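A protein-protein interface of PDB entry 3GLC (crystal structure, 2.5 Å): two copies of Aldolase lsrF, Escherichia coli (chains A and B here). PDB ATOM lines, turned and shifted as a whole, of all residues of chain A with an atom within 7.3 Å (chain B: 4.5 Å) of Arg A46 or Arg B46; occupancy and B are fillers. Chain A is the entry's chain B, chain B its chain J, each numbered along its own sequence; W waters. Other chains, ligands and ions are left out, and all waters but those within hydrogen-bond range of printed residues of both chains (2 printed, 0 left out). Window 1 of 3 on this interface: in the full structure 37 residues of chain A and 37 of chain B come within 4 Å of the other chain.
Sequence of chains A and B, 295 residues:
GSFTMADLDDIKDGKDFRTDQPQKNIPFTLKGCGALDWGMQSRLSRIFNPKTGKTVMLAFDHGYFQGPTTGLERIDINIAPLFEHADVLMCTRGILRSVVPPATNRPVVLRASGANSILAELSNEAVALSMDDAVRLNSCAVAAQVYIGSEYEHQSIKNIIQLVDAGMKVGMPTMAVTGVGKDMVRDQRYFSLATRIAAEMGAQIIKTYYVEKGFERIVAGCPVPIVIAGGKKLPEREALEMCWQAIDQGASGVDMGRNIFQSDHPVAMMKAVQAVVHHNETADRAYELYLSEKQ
Water W1 lies within hydrogen-bond range of the backbone carbonyl oxygen of Ser A42 (2.7 Å) and the side-chain amide oxygen of Asn B105 (2.9 Å).
Water W2 bridges the side-chain hydroxyl of Ser A42 (3.1 Å) and the backbone NH of Asn B105 (3.3 Å).
Of chain B, only Arg B46 and Asn B105 come within 4 Å of Arg A46.
Of the printed residues of chain A, Arg B46 touches Arg A46 and Asn A105.
Of the printed residues of chain A, Asn B105 touches Ser A45 (3.5 Å) and Arg A46 (3.5 Å).
Of the printed residues of chain A, Asn B138 touches Ser A42, Arg A43 and Asn A138.
The nearest printed residue of chain B that does not touch Arg A46 is Asn B138 (4.5 Å).
The nearest residue of chain A that does not touch Arg B46 is Asn A138 (4.4 Å).
Among the printed residues, merely in contact across the chains: Ser A45 with Asn B105, Arg A46 with Arg B46, Arg A46 with Asn B105, Pro A102 with Ser B45, Asn A105 with Ser B45, Asn A105 with Arg B46, Asn A138 with Arg B43 and Asn A138 with Asn B138.
Ser A42 touches Asn B138, and with the chains exchanged Asn A138 touches Ser B42.
Arg A43 touches Asn B138, and with the chains exchanged Asn A138 touches Arg B43.
Arg B46 touches its own counterpart, Arg A46.
Asn B138 touches its own counterpart, Asn A138.
12 positions are printed for both chains.
Of the 11 pairs that touch across the chains among the printed residues, 10 have their exchanged pair printed and touching as well.
The side-chain amide oxygen of Asn B138 is in hydrogen-bond range of the guanidinium group of Arg A43 (3.3 Å).
The side-chain hydroxyl of Ser B42 sits at hydrogen-bond distance from the side-chain amide nitrogen of Asn A138 (3.4 Å).
ND2 of Asn B138 is in hydrogen-bond range of OG of Ser A42 (3.3 Å).
The guanidinium group (NH1) of Arg B46 is in hydrogen-bond range of the side-chain sulfur (SG) of Cys B140 (3.8 Å).
O of Ser A139 sits at hydrogen-bond distance from NE of Arg A43.
The backbone carbonyl oxygen of Gln A41 lies within hydrogen-bond range of the side-chain hydroxyl of Ser A45, 2.9 Å away.
Printed residues of chain B that touch a printed residue of chain A: Ser B42, Arg B43, Ser B45, Arg B46, Asn B105 and Asn B138.
Along chain B the printed residues that touch a printed residue of chain A span positions 42 to 138.
Along chain A the printed residues that touch a printed residue of chain B span positions 42 to 138.
Among the printed residues, 11 pairs touch across the chains.
Among the printed residues, no Asp or Glu carboxylate lies within 4 Å of a Lys or Arg side-chain nitrogen of the other chain.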
ATOM      1  N   MET A  40       9.746 -16.326 -21.786  1.00  0.00           N
ATOM      2  CA  MET A  40      10.202 -16.485 -23.126  1.00  0.00           C
ATOM      3  C   MET A  40      11.305 -17.551 -23.170  1.00  0.00           C
ATOM      4  O   MET A  40      11.311 -18.432 -24.043  1.00  0.00           O
ATOM      5  CB  MET A  40      10.726 -15.171 -23.663  1.00  0.00           C
ATOM      6  CG  MET A  40      10.864 -15.241 -25.157  1.00  0.00           C
ATOM      7  SD  MET A  40      10.932 -13.656 -25.988  1.00  0.00           S
ATOM      8  CE  MET A  40       9.343 -12.946 -25.777  1.00  0.00           C
ATOM      9  N   GLN A  41      12.243 -17.459 -22.226  1.00  0.00           N
ATOM     10  CA  GLN A  41      13.342 -18.430 -22.130  1.00  0.00           C
ATOM     11  C   GLN A  41      12.768 -19.804 -21.922  1.00  0.00           C
ATOM     12  O   GLN A  41      13.248 -20.772 -22.477  1.00  0.00           O
ATOM     13  CB  GLN A  41      14.312 -18.076 -21.020  1.00  0.00           C
ATOM     14  CG  GLN A  41      15.123 -16.833 -21.356  1.00  0.00           C
ATOM     15  CD  GLN A  41      16.155 -16.473 -20.296  1.00  0.00           C
ATOM     16  OE1 GLN A  41      15.979 -16.749 -19.115  1.00  0.00           O
ATOM     17  NE2 GLN A  41      17.208 -15.822 -20.712  1.00  0.00           N
ATOM     18  N   SER A  42      11.682 -19.875 -21.184  1.00  0.00           N
ATOM     19  CA  SER A  42      11.034 -21.150 -20.921  1.00  0.00           C
ATOM     20  C   SER A  42      10.448 -21.769 -22.193  1.00  0.00           C
ATOM     21  O   SER A  42      10.594 -22.976 -22.424  1.00  0.00           O
ATOM     22  CB  SER A  42       9.980 -20.970 -19.828  1.00  0.00           C
ATOM     23  OG  SER A  42       9.112 -22.078 -19.801  1.00  0.00           O
ATOM     24  N   ARG A  43       9.787 -20.948 -23.009  1.00  0.00           N
ATOM     25  CA  ARG A  43       9.220 -21.407 -24.270  1.00  0.00           C
ATOM     26  C   ARG A  43      10.336 -21.834 -25.226  1.00  0.00           C
ATOM     27  O   ARG A  43      10.198 -22.838 -25.927  1.00  0.00           O
ATOM     28  CB  ARG A  43       8.346 -20.310 -24.929  1.00  0.00           C
ATOM     29  CG  ARG A  43       7.039 -20.084 -24.282  1.00  0.00           C
ATOM     30  CD  ARG A  43       6.136 -19.181 -25.071  1.00  0.00           C
ATOM     31  NE  ARG A  43       4.828 -19.067 -24.397  1.00  0.00           N
ATOM     32  CZ  ARG A  43       4.495 -18.129 -23.502  1.00  0.00           C
ATOM     33  NH1 ARG A  43       5.358 -17.155 -23.151  1.00  0.00           N
ATOM     34  NH2 ARG A  43       3.281 -18.159 -22.954  1.00  0.00           N
ATOM     35  N   LEU A  44      11.430 -21.072 -25.253  1.00  0.00           N
ATOM     36  CA  LEU A  44      12.575 -21.415 -26.098  1.00  0.00           C
ATOM     37  C   LEU A  44      13.278 -22.710 -25.639  1.00  0.00           C
ATOM     38  O   LEU A  44      13.742 -23.493 -26.462  1.00  0.00           O
ATOM     39  CB  LEU A  44      13.576 -20.280 -26.129  1.00  0.00           C
ATOM     40  CG  LEU A  44      13.213 -19.031 -26.943  1.00  0.00           C
ATOM     41  CD1 LEU A  44      14.113 -17.884 -26.564  1.00  0.00           C
ATOM     42  CD2 LEU A  44      13.265 -19.285 -28.467  1.00  0.00           C
ATOM     43  N   SER A  45      13.309 -22.958 -24.333  1.00  0.00           N
ATOM     44  CA  SER A  45      13.765 -24.245 -23.826  1.00  0.00           C
ATOM     45  C   SER A  45      12.867 -25.453 -24.176  1.00  0.00           C
ATOM     46  O   SER A  45      13.325 -26.586 -24.075  1.00  0.00           O
ATOM     47  CB  SER A  45      13.984 -24.170 -22.327  1.00  0.00           C
ATOM     48  OG  SER A  45      14.881 -23.112 -22.015  1.00  0.00           O
ATOM     49  N   ARG A  46      11.616 -25.241 -24.562  1.00  0.00           N
ATOM     50  CA  ARG A  46      10.819 -26.350 -24.998  1.00  0.00           C
ATOM     51  C   ARG A  46      11.195 -26.717 -26.410  1.00  0.00           C
ATOM     52  O   ARG A  46      10.993 -27.851 -26.825  1.00  0.00           O
ATOM     53  CB  ARG A  46       9.320 -26.016 -24.937  1.00  0.00           C
ATOM     54  CG  ARG A  46       8.773 -25.937 -23.512  1.00  0.00           C
ATOM     55  CD  ARG A  46       7.270 -26.018 -23.494  1.00  0.00           C
ATOM     56  NE  ARG A  46       6.780 -27.349 -23.834  1.00  0.00           N
ATOM     57  CZ  ARG A  46       5.533 -27.589 -24.240  1.00  0.00           C
ATOM     58  NH1 ARG A  46       4.658 -26.592 -24.356  1.00  0.00           N
ATOM     59  NH2 ARG A  46       5.153 -28.820 -24.543  1.00  0.00           N
ATOM     60  N   ILE A  47      11.719 -25.749 -27.159  1.00  0.00           N
ATOM     61  CA  ILE A  47      12.018 -25.964 -28.572  1.00  0.00           C
ATOM     62  C   ILE A  47      13.437 -26.502 -28.733  1.00  0.00           C
ATOM     63  O   ILE A  47      13.644 -27.534 -29.374  1.00  0.00           O
ATOM     64  CB  ILE A  47      11.876 -24.675 -29.398  1.00  0.00           C
ATOM     65  CG1 ILE A  47      10.420 -24.231 -29.465  1.00  0.00           C
ATOM     66  CG2 ILE A  47      12.389 -24.885 -30.815  1.00  0.00           C
ATOM     67  CD1 ILE A  47      10.164 -22.722 -29.988  1.00  0.00           C
ATOM     68  N   PHE A  48      14.407 -25.786 -28.163  1.00  0.00           N
ATOM     69  CA  PHE A  48      15.817 -26.196 -28.166  1.00  0.00           C
ATOM     70  C   PHE A  48      16.200 -26.877 -26.872  1.00  0.00           C
ATOM     71  O   PHE A  48      16.232 -26.228 -25.827  1.00  0.00           O
ATOM     72  CB  PHE A  48      16.716 -24.973 -28.352  1.00  0.00           C
ATOM     73  CG  PHE A  48      16.402 -24.180 -29.588  1.00  0.00           C
ATOM     74  CD1 PHE A  48      16.930 -24.559 -30.820  1.00  0.00           C
ATOM     75  CD2 PHE A  48      15.560 -23.069 -29.530  1.00  0.00           C
ATOM     76  CE1 PHE A  48      16.620 -23.837 -31.983  1.00  0.00           C
ATOM     77  CE2 PHE A  48      15.254 -22.334 -30.688  1.00  0.00           C
ATOM     78  CZ  PHE A  48      15.791 -22.717 -31.909  1.00  0.00           C
ATOM     79  N   ASN A  49      16.491 -28.177 -26.952  1.00  0.00           N
ATOM     80  CA  ASN A  49      16.894 -28.969 -25.801  1.00  0.00           C
ATOM     81  C   ASN A  49      18.043 -28.267 -25.079  1.00  0.00           C
ATOM     82  O   ASN A  49      19.053 -27.981 -25.695  1.00  0.00           O
ATOM     83  CB  ASN A  49      17.296 -30.354 -26.283  1.00  0.00           C
ATOM     84  CG  ASN A  49      17.810 -31.227 -25.177  1.00  0.00           C
ATOM     85  OD1 ASN A  49      18.870 -30.983 -24.598  1.00  0.00           O
ATOM     86  ND2 ASN A  49      17.067 -32.268 -24.882  1.00  0.00           N
ATOM     87  N   PRO A  50      17.888 -27.972 -23.774  1.00  0.00           N
ATOM     88  CA  PRO A  50      18.906 -27.242 -22.990  1.00  0.00           C
ATOM     89  C   PRO A  50      20.277 -27.935 -22.925  1.00  0.00           C
ATOM     90  O   PRO A  50      21.315 -27.241 -22.903  1.00  0.00           O
ATOM     91  CB  PRO A  50      18.318 -27.193 -21.580  1.00  0.00           C
ATOM     92  CG  PRO A  50      16.874 -27.571 -21.717  1.00  0.00           C
ATOM     93  CD  PRO A  50      16.758 -28.424 -22.940  1.00  0.00           C
ATOM     94  N   LYS A  54      19.980 -27.747 -29.339  1.00  0.00           N
ATOM     95  CA  LYS A  54      19.523 -28.054 -30.689  1.00  0.00           C
ATOM     96  C   LYS A  54      18.107 -28.592 -30.716  1.00  0.00           C
ATOM     97  O   LYS A  54      17.578 -28.985 -29.671  1.00  0.00           O
ATOM     98  CB  LYS A  54      20.466 -29.040 -31.375  1.00  0.00           C
ATOM     99  CG  LYS A  54      21.842 -28.473 -31.635  1.00  0.00           C
ATOM    100  CD  LYS A  54      22.846 -29.609 -31.746  1.00  0.00           C
ATOM    101  CE  LYS A  54      24.309 -29.125 -31.666  1.00  0.00           C
ATOM    102  NZ  LYS A  54      24.509 -27.861 -32.469  1.00  0.00           N
ATOM    103  N   THR A  55      17.508 -28.605 -31.913  1.00  0.00           N
ATOM    104  CA  THR A  55      16.133 -29.031 -32.091  1.00  0.00           C
ATOM    105  C   THR A  55      15.920 -29.783 -33.377  1.00  0.00           C
ATOM    106  O   THR A  55      16.538 -29.481 -34.391  1.00  0.00           O
ATOM    107  CB  THR A  55      15.153 -27.799 -32.099  1.00  0.00           C
ATOM    108  OG1 THR A  55      13.815 -28.253 -31.885  1.00  0.00           O
ATOM    109  CG2 THR A  55      15.196 -26.996 -33.419  1.00  0.00           C
ATOM    110  N   ASP A  87      10.905 -33.290 -31.845  1.00  0.00           N
ATOM    111  CA  ASP A  87      11.065 -32.425 -30.681  1.00  0.00           C
ATOM    112  C   ASP A  87       9.925 -31.415 -30.641  1.00  0.00           C
ATOM    113  O   ASP A  87       9.355 -31.154 -29.575  1.00  0.00           O
ATOM    114  CB  ASP A  87      12.400 -31.678 -30.716  1.00  0.00           C
ATOM    115  CG  ASP A  87      13.616 -32.601 -30.473  1.00  0.00           C
ATOM    116  OD1 ASP A  87      13.463 -33.704 -29.898  1.00  0.00           O
ATOM    117  OD2 ASP A  87      14.741 -32.219 -30.849  1.00  0.00           O
ATOM    118  N   VAL A  88       9.595 -30.847 -31.800  1.00  0.00           N
ATOM    119  CA  VAL A  88       8.624 -29.754 -31.885  1.00  0.00           C
ATOM    120  C   VAL A  88       7.877 -29.839 -33.195  1.00  0.00           C
ATOM    121  O   VAL A  88       8.480 -30.179 -34.209  1.00  0.00           O
ATOM    122  CB  VAL A  88       9.269 -28.360 -31.672  1.00  0.00           C
ATOM    123  CG1 VAL A  88      10.656 -28.343 -32.149  1.00  0.00           C
ATOM    124  CG2 VAL A  88       8.488 -27.293 -32.381  1.00  0.00           C
ATOM    125  N   PRO A 102      -4.494 -32.994 -28.894  1.00  0.00           N
ATOM    126  CA  PRO A 102      -3.771 -32.249 -27.845  1.00  0.00           C
ATOM    127  C   PRO A 102      -2.970 -33.158 -26.933  1.00  0.00           C
ATOM    128  O   PRO A 102      -2.042 -32.692 -26.285  1.00  0.00           O
ATOM    129  CB  PRO A 102      -4.893 -31.565 -27.054  1.00  0.00           C
ATOM    130  CG  PRO A 102      -6.169 -32.235 -27.532  1.00  0.00           C
ATOM    131  CD  PRO A 102      -5.936 -32.680 -28.921  1.00  0.00           C
ATOM    132  N   ASN A 105       1.173 -33.835 -26.598  1.00  0.00           N
ATOM    133  CA  ASN A 105       2.120 -33.300 -25.595  1.00  0.00           C
ATOM    134  C   ASN A 105       3.478 -32.979 -26.166  1.00  0.00           C
ATOM    135  O   ASN A 105       4.504 -33.388 -25.623  1.00  0.00           O
ATOM    136  CB  ASN A 105       2.281 -34.259 -24.398  1.00  0.00           C
ATOM    137  CG  ASN A 105       2.983 -33.599 -23.213  1.00  0.00           C
ATOM    138  OD1 ASN A 105       3.084 -32.367 -23.130  1.00  0.00           O
ATOM    139  ND2 ASN A 105       3.487 -34.409 -22.300  1.00  0.00           N
ATOM    140  N   ARG A 106       3.490 -32.237 -27.269  1.00  0.00           N
ATOM    141  CA  ARG A 106       4.716 -31.857 -27.984  1.00  0.00           C
ATOM    142  C   ARG A 106       4.596 -30.346 -28.233  1.00  0.00           C
ATOM    143  O   ARG A 106       3.508 -29.857 -28.576  1.00  0.00           O
ATOM    144  CB  ARG A 106       4.723 -32.626 -29.289  1.00  0.00           C
ATOM    145  CG  ARG A 106       6.015 -33.206 -29.746  1.00  0.00           C
ATOM    146  CD  ARG A 106       6.858 -33.917 -28.665  1.00  0.00           C
ATOM    147  NE  ARG A 106       6.300 -35.190 -28.269  1.00  0.00           N
ATOM    148  CZ  ARG A 106       6.996 -36.167 -27.716  1.00  0.00           C
ATOM    149  NH1 ARG A 106       8.287 -36.020 -27.505  1.00  0.00           N
ATOM    150  NH2 ARG A 106       6.410 -37.303 -27.382  1.00  0.00           N
ATOM    151  N   PRO A 107       5.689 -29.591 -28.015  1.00  0.00           N
ATOM    152  CA  PRO A 107       5.711 -28.147 -28.279  1.00  0.00           C
ATOM    153  C   PRO A 107       5.307 -27.824 -29.719  1.00  0.00           C
ATOM    154  O   PRO A 107       5.685 -28.572 -30.659  1.00  0.00           O
ATOM    155  CB  PRO A 107       7.178 -27.774 -28.098  1.00  0.00           C
ATOM    156  CG  PRO A 107       7.783 -28.864 -27.308  1.00  0.00           C
ATOM    157  CD  PRO A 107       6.948 -30.091 -27.423  1.00  0.00           C
ATOM    158  N   VAL A 108       4.559 -26.721 -29.918  1.00  0.00           N
ATOM    159  CA  VAL A 108       4.200 -26.338 -31.278  1.00  0.00           C
ATOM    160  C   VAL A 108       4.635 -24.912 -31.621  1.00  0.00           C
ATOM    161  O   VAL A 108       4.604 -23.989 -30.783  1.00  0.00           O
ATOM    162  CB  VAL A 108       2.694 -26.529 -31.612  1.00  0.00           C
ATOM    163  CG1 VAL A 108       2.135 -27.856 -31.098  1.00  0.00           C
ATOM    164  CG2 VAL A 108       1.910 -25.429 -31.001  1.00  0.00           C
ATOM    165  N   ASN A 138      -1.531 -22.132 -26.591  1.00  0.00           N
ATOM    166  CA  ASN A 138      -0.344 -22.514 -25.834  1.00  0.00           C
ATOM    167  C   ASN A 138       0.882 -22.789 -26.723  1.00  0.00           C
ATOM    168  O   ASN A 138       1.602 -23.764 -26.484  1.00  0.00           O
ATOM    169  CB  ASN A 138      -0.626 -23.762 -24.981  1.00  0.00           C
ATOM    170  CG  ASN A 138       0.557 -24.144 -24.088  1.00  0.00           C
ATOM    171  OD1 ASN A 138       1.288 -23.272 -23.613  1.00  0.00           O
ATOM    172  ND2 ASN A 138       0.738 -25.447 -23.840  1.00  0.00           N
ATOM    173  N   SER A 139       1.106 -21.944 -27.730  1.00  0.00           N
ATOM    174  CA  SER A 139       2.245 -22.066 -28.624  1.00  0.00           C
ATOM    175  C   SER A 139       3.519 -21.791 -27.865  1.00  0.00           C
ATOM    176  O   SER A 139       3.507 -21.097 -26.817  1.00  0.00           O
ATOM    177  CB  SER A 139       2.203 -21.024 -29.721  1.00  0.00           C
ATOM    178  OG  SER A 139       0.906 -20.875 -30.203  1.00  0.00           O
ATOM    179  N   CYS A 140       4.616 -22.297 -28.426  1.00  0.00           N
ATOM    180  CA  CYS A 140       5.944 -21.931 -27.982  1.00  0.00           C
ATOM    181  C   CYS A 140       6.514 -20.785 -28.774  1.00  0.00           C
ATOM    182  O   CYS A 140       7.349 -20.060 -28.279  1.00  0.00           O
ATOM    183  CB  CYS A 140       6.877 -23.121 -28.109  1.00  0.00           C
ATOM    184  SG  CYS A 140       6.380 -24.452 -27.054  1.00  0.00           S
ATOM    185  N   SER B  42      -4.105 -28.785 -24.043  1.00  0.00           N
ATOM    186  CA  SER B  42      -2.657 -28.943 -24.212  1.00  0.00           C
ATOM    187  C   SER B  42      -1.953 -28.628 -22.906  1.00  0.00           C
ATOM    188  O   SER B  42      -1.100 -29.389 -22.477  1.00  0.00           O
ATOM    189  CB  SER B  42      -2.194 -28.058 -25.346  1.00  0.00           C
ATOM    190  OG  SER B  42      -0.795 -28.000 -25.413  1.00  0.00           O
ATOM    191  N   ARG B  43      -2.346 -27.555 -22.224  1.00  0.00           N
ATOM    192  CA  ARG B  43      -1.727 -27.220 -20.940  1.00  0.00           C
ATOM    193  C   ARG B  43      -1.981 -28.315 -19.911  1.00  0.00           C
ATOM    194  O   ARG B  43      -1.115 -28.648 -19.072  1.00  0.00           O
ATOM    195  CB  ARG B  43      -2.214 -25.870 -20.427  1.00  0.00           C
ATOM    196  CG  ARG B  43      -1.603 -24.672 -21.177  1.00  0.00           C
ATOM    197  CD  ARG B  43      -1.931 -23.337 -20.505  1.00  0.00           C
ATOM    198  NE  ARG B  43      -1.289 -22.261 -21.258  1.00  0.00           N
ATOM    199  CZ  ARG B  43      -1.878 -21.562 -22.241  1.00  0.00           C
ATOM    200  NH1 ARG B  43      -3.161 -21.769 -22.565  1.00  0.00           N
ATOM    201  NH2 ARG B  43      -1.191 -20.640 -22.901  1.00  0.00           N
ATOM    202  N   LEU B  44      -3.153 -28.916 -19.983  1.00  0.00           N
ATOM    203  CA  LEU B  44      -3.507 -29.909 -18.996  1.00  0.00           C
ATOM    204  C   LEU B  44      -2.694 -31.183 -19.247  1.00  0.00           C
ATOM    205  O   LEU B  44      -2.347 -31.890 -18.305  1.00  0.00           O
ATOM    206  CB  LEU B  44      -5.015 -30.165 -19.016  1.00  0.00           C
ATOM    207  CG  LEU B  44      -5.905 -29.136 -18.320  1.00  0.00           C
ATOM    208  CD1 LEU B  44      -7.337 -29.361 -18.700  1.00  0.00           C
ATOM    209  CD2 LEU B  44      -5.774 -29.166 -16.805  1.00  0.00           C
ATOM    210  N   SER B  45      -2.377 -31.431 -20.515  1.00  0.00           N
ATOM    211  CA  SER B  45      -1.585 -32.586 -20.885  1.00  0.00           C
ATOM    212  C   SER B  45      -0.129 -32.459 -20.520  1.00  0.00           C
ATOM    213  O   SER B  45       0.569 -33.448 -20.509  1.00  0.00           O
ATOM    214  CB  SER B  45      -1.693 -32.881 -22.354  1.00  0.00           C
ATOM    215  OG  SER B  45      -2.984 -33.293 -22.640  1.00  0.00           O
ATOM    216  N   ARG B  46       0.353 -31.252 -20.256  1.00  0.00           N
ATOM    217  CA  ARG B  46       1.704 -31.097 -19.745  1.00  0.00           C
ATOM    218  C   ARG B  46       1.735 -31.481 -18.262  1.00  0.00           C
ATOM    219  O   ARG B  46       2.784 -31.881 -17.752  1.00  0.00           O
ATOM    220  CB  ARG B  46       2.225 -29.669 -19.914  1.00  0.00           C
ATOM    221  CG  ARG B  46       2.464 -29.279 -21.366  1.00  0.00           C
ATOM    222  CD  ARG B  46       3.312 -28.052 -21.409  1.00  0.00           C
ATOM    223  NE  ARG B  46       4.709 -28.312 -21.029  1.00  0.00           N
ATOM    224  CZ  ARG B  46       5.563 -27.357 -20.663  1.00  0.00           C
ATOM    225  NH1 ARG B  46       5.167 -26.093 -20.599  1.00  0.00           N
ATOM    226  NH2 ARG B  46       6.800 -27.657 -20.341  1.00  0.00           N
ATOM    227  N   ILE B  47       0.585 -31.344 -17.592  1.00  0.00           N
ATOM    228  CA  ILE B  47       0.486 -31.609 -16.171  1.00  0.00           C
ATOM    229  C   ILE B  47       0.211 -33.093 -15.904  1.00  0.00           C
ATOM    230  O   ILE B  47       0.941 -33.736 -15.145  1.00  0.00           O
ATOM    231  CB  ILE B  47      -0.591 -30.739 -15.501  1.00  0.00           C
ATOM    232  CG1 ILE B  47      -0.142 -29.294 -15.499  1.00  0.00           C
ATOM    233  CG2 ILE B  47      -0.780 -31.171 -14.055  1.00  0.00           C
ATOM    234  CD1 ILE B  47      -1.243 -28.285 -15.089  1.00  0.00           C
ATOM    235  N   PHE B  48      -0.854 -33.608 -16.517  1.00  0.00           N
ATOM    236  CA  PHE B  48      -1.255 -34.992 -16.364  1.00  0.00           C
ATOM    237  C   PHE B  48      -0.801 -35.739 -17.581  1.00  0.00           C
ATOM    238  O   PHE B  48      -1.271 -35.461 -18.696  1.00  0.00           O
ATOM    239  CB  PHE B  48      -2.772 -35.115 -16.220  1.00  0.00           C
ATOM    240  CG  PHE B  48      -3.325 -34.332 -15.066  1.00  0.00           C
ATOM    241  CD1 PHE B  48      -3.354 -34.885 -13.777  1.00  0.00           C
ATOM    242  CD2 PHE B  48      -3.782 -33.026 -15.244  1.00  0.00           C
ATOM    243  CE1 PHE B  48      -3.839 -34.130 -12.669  1.00  0.00           C
ATOM    244  CE2 PHE B  48      -4.282 -32.254 -14.141  1.00  0.00           C
ATOM    245  CZ  PHE B  48      -4.310 -32.798 -12.870  1.00  0.00           C
ATOM    246  N   ASN B 105      13.086 -26.710 -17.978  1.00  0.00           N
ATOM    247  CA  ASN B 105      12.166 -27.300 -18.947  1.00  0.00           C
ATOM    248  C   ASN B 105      11.156 -28.238 -18.326  1.00  0.00           C
ATOM    249  O   ASN B 105      10.984 -29.350 -18.781  1.00  0.00           O
ATOM    250  CB  ASN B 105      12.935 -28.023 -20.048  1.00  0.00           C
ATOM    251  CG  ASN B 105      12.051 -28.390 -21.244  1.00  0.00           C
ATOM    252  OD1 ASN B 105      10.981 -27.815 -21.465  1.00  0.00           O
ATOM    253  ND2 ASN B 105      12.509 -29.347 -22.030  1.00  0.00           N
ATOM    254  N   ARG B 106      10.467 -27.745 -17.307  1.00  0.00           N
ATOM    255  CA  ARG B 106       9.483 -28.507 -16.563  1.00  0.00           C
ATOM    256  C   ARG B 106       8.218 -27.628 -16.416  1.00  0.00           C
ATOM    257  O   ARG B 106       8.349 -26.429 -16.195  1.00  0.00           O
ATOM    258  CB  ARG B 106      10.125 -28.831 -15.207  1.00  0.00           C
ATOM    259  CG  ARG B 106       9.831 -30.193 -14.615  1.00  0.00           C
ATOM    260  CD  ARG B 106      10.027 -31.344 -15.603  1.00  0.00           C
ATOM    261  NE  ARG B 106      11.434 -31.601 -15.844  1.00  0.00           N
ATOM    262  CZ  ARG B 106      11.902 -32.756 -16.279  1.00  0.00           C
ATOM    263  NH1 ARG B 106      11.067 -33.761 -16.494  1.00  0.00           N
ATOM    264  NH2 ARG B 106      13.198 -32.917 -16.462  1.00  0.00           N
ATOM    265  N   PRO B 107       7.006 -28.210 -16.600  1.00  0.00           N
ATOM    266  CA  PRO B 107       5.765 -27.420 -16.549  1.00  0.00           C
ATOM    267  C   PRO B 107       5.602 -26.808 -15.161  1.00  0.00           C
ATOM    268  O   PRO B 107       5.931 -27.483 -14.168  1.00  0.00           O
ATOM    269  CB  PRO B 107       4.652 -28.459 -16.777  1.00  0.00           C
ATOM    270  CG  PRO B 107       5.271 -29.699 -17.224  1.00  0.00           C
ATOM    271  CD  PRO B 107       6.787 -29.594 -17.070  1.00  0.00           C
ATOM    272  N   ASN B 138       4.648 -18.277 -19.127  1.00  0.00           N
ATOM    273  CA  ASN B 138       4.339 -19.552 -19.735  1.00  0.00           C
ATOM    274  C   ASN B 138       3.840 -20.635 -18.744  1.00  0.00           C
ATOM    275  O   ASN B 138       4.238 -21.797 -18.871  1.00  0.00           O
ATOM    276  CB  ASN B 138       5.568 -20.020 -20.504  1.00  0.00           C
ATOM    277  CG  ASN B 138       5.298 -21.201 -21.407  1.00  0.00           C
ATOM    278  OD1 ASN B 138       4.266 -21.292 -22.057  1.00  0.00           O
ATOM    279  ND2 ASN B 138       6.261 -22.131 -21.442  1.00  0.00           N
ATOM    280  N   CYS B 140       1.334 -23.376 -16.891  1.00  0.00           N
ATOM    281  CA  CYS B 140       0.375 -24.375 -17.322  1.00  0.00           C
ATOM    282  C   CYS B 140      -0.914 -24.252 -16.611  1.00  0.00           C
ATOM    283  O   CYS B 140      -1.909 -24.736 -17.111  1.00  0.00           O
ATOM    284  CB  CYS B 140       0.931 -25.774 -17.085  1.00  0.00           C
ATOM    285  SG  CYS B 140       2.288 -26.063 -18.166  1.00  0.00           S
HETATM  286  O   HOH W   1      10.433 -25.087 -20.808  1.00  0.00           O
HETATM  287  O   HOH W   2      11.098 -24.124 -18.505  1.00  0.00           O
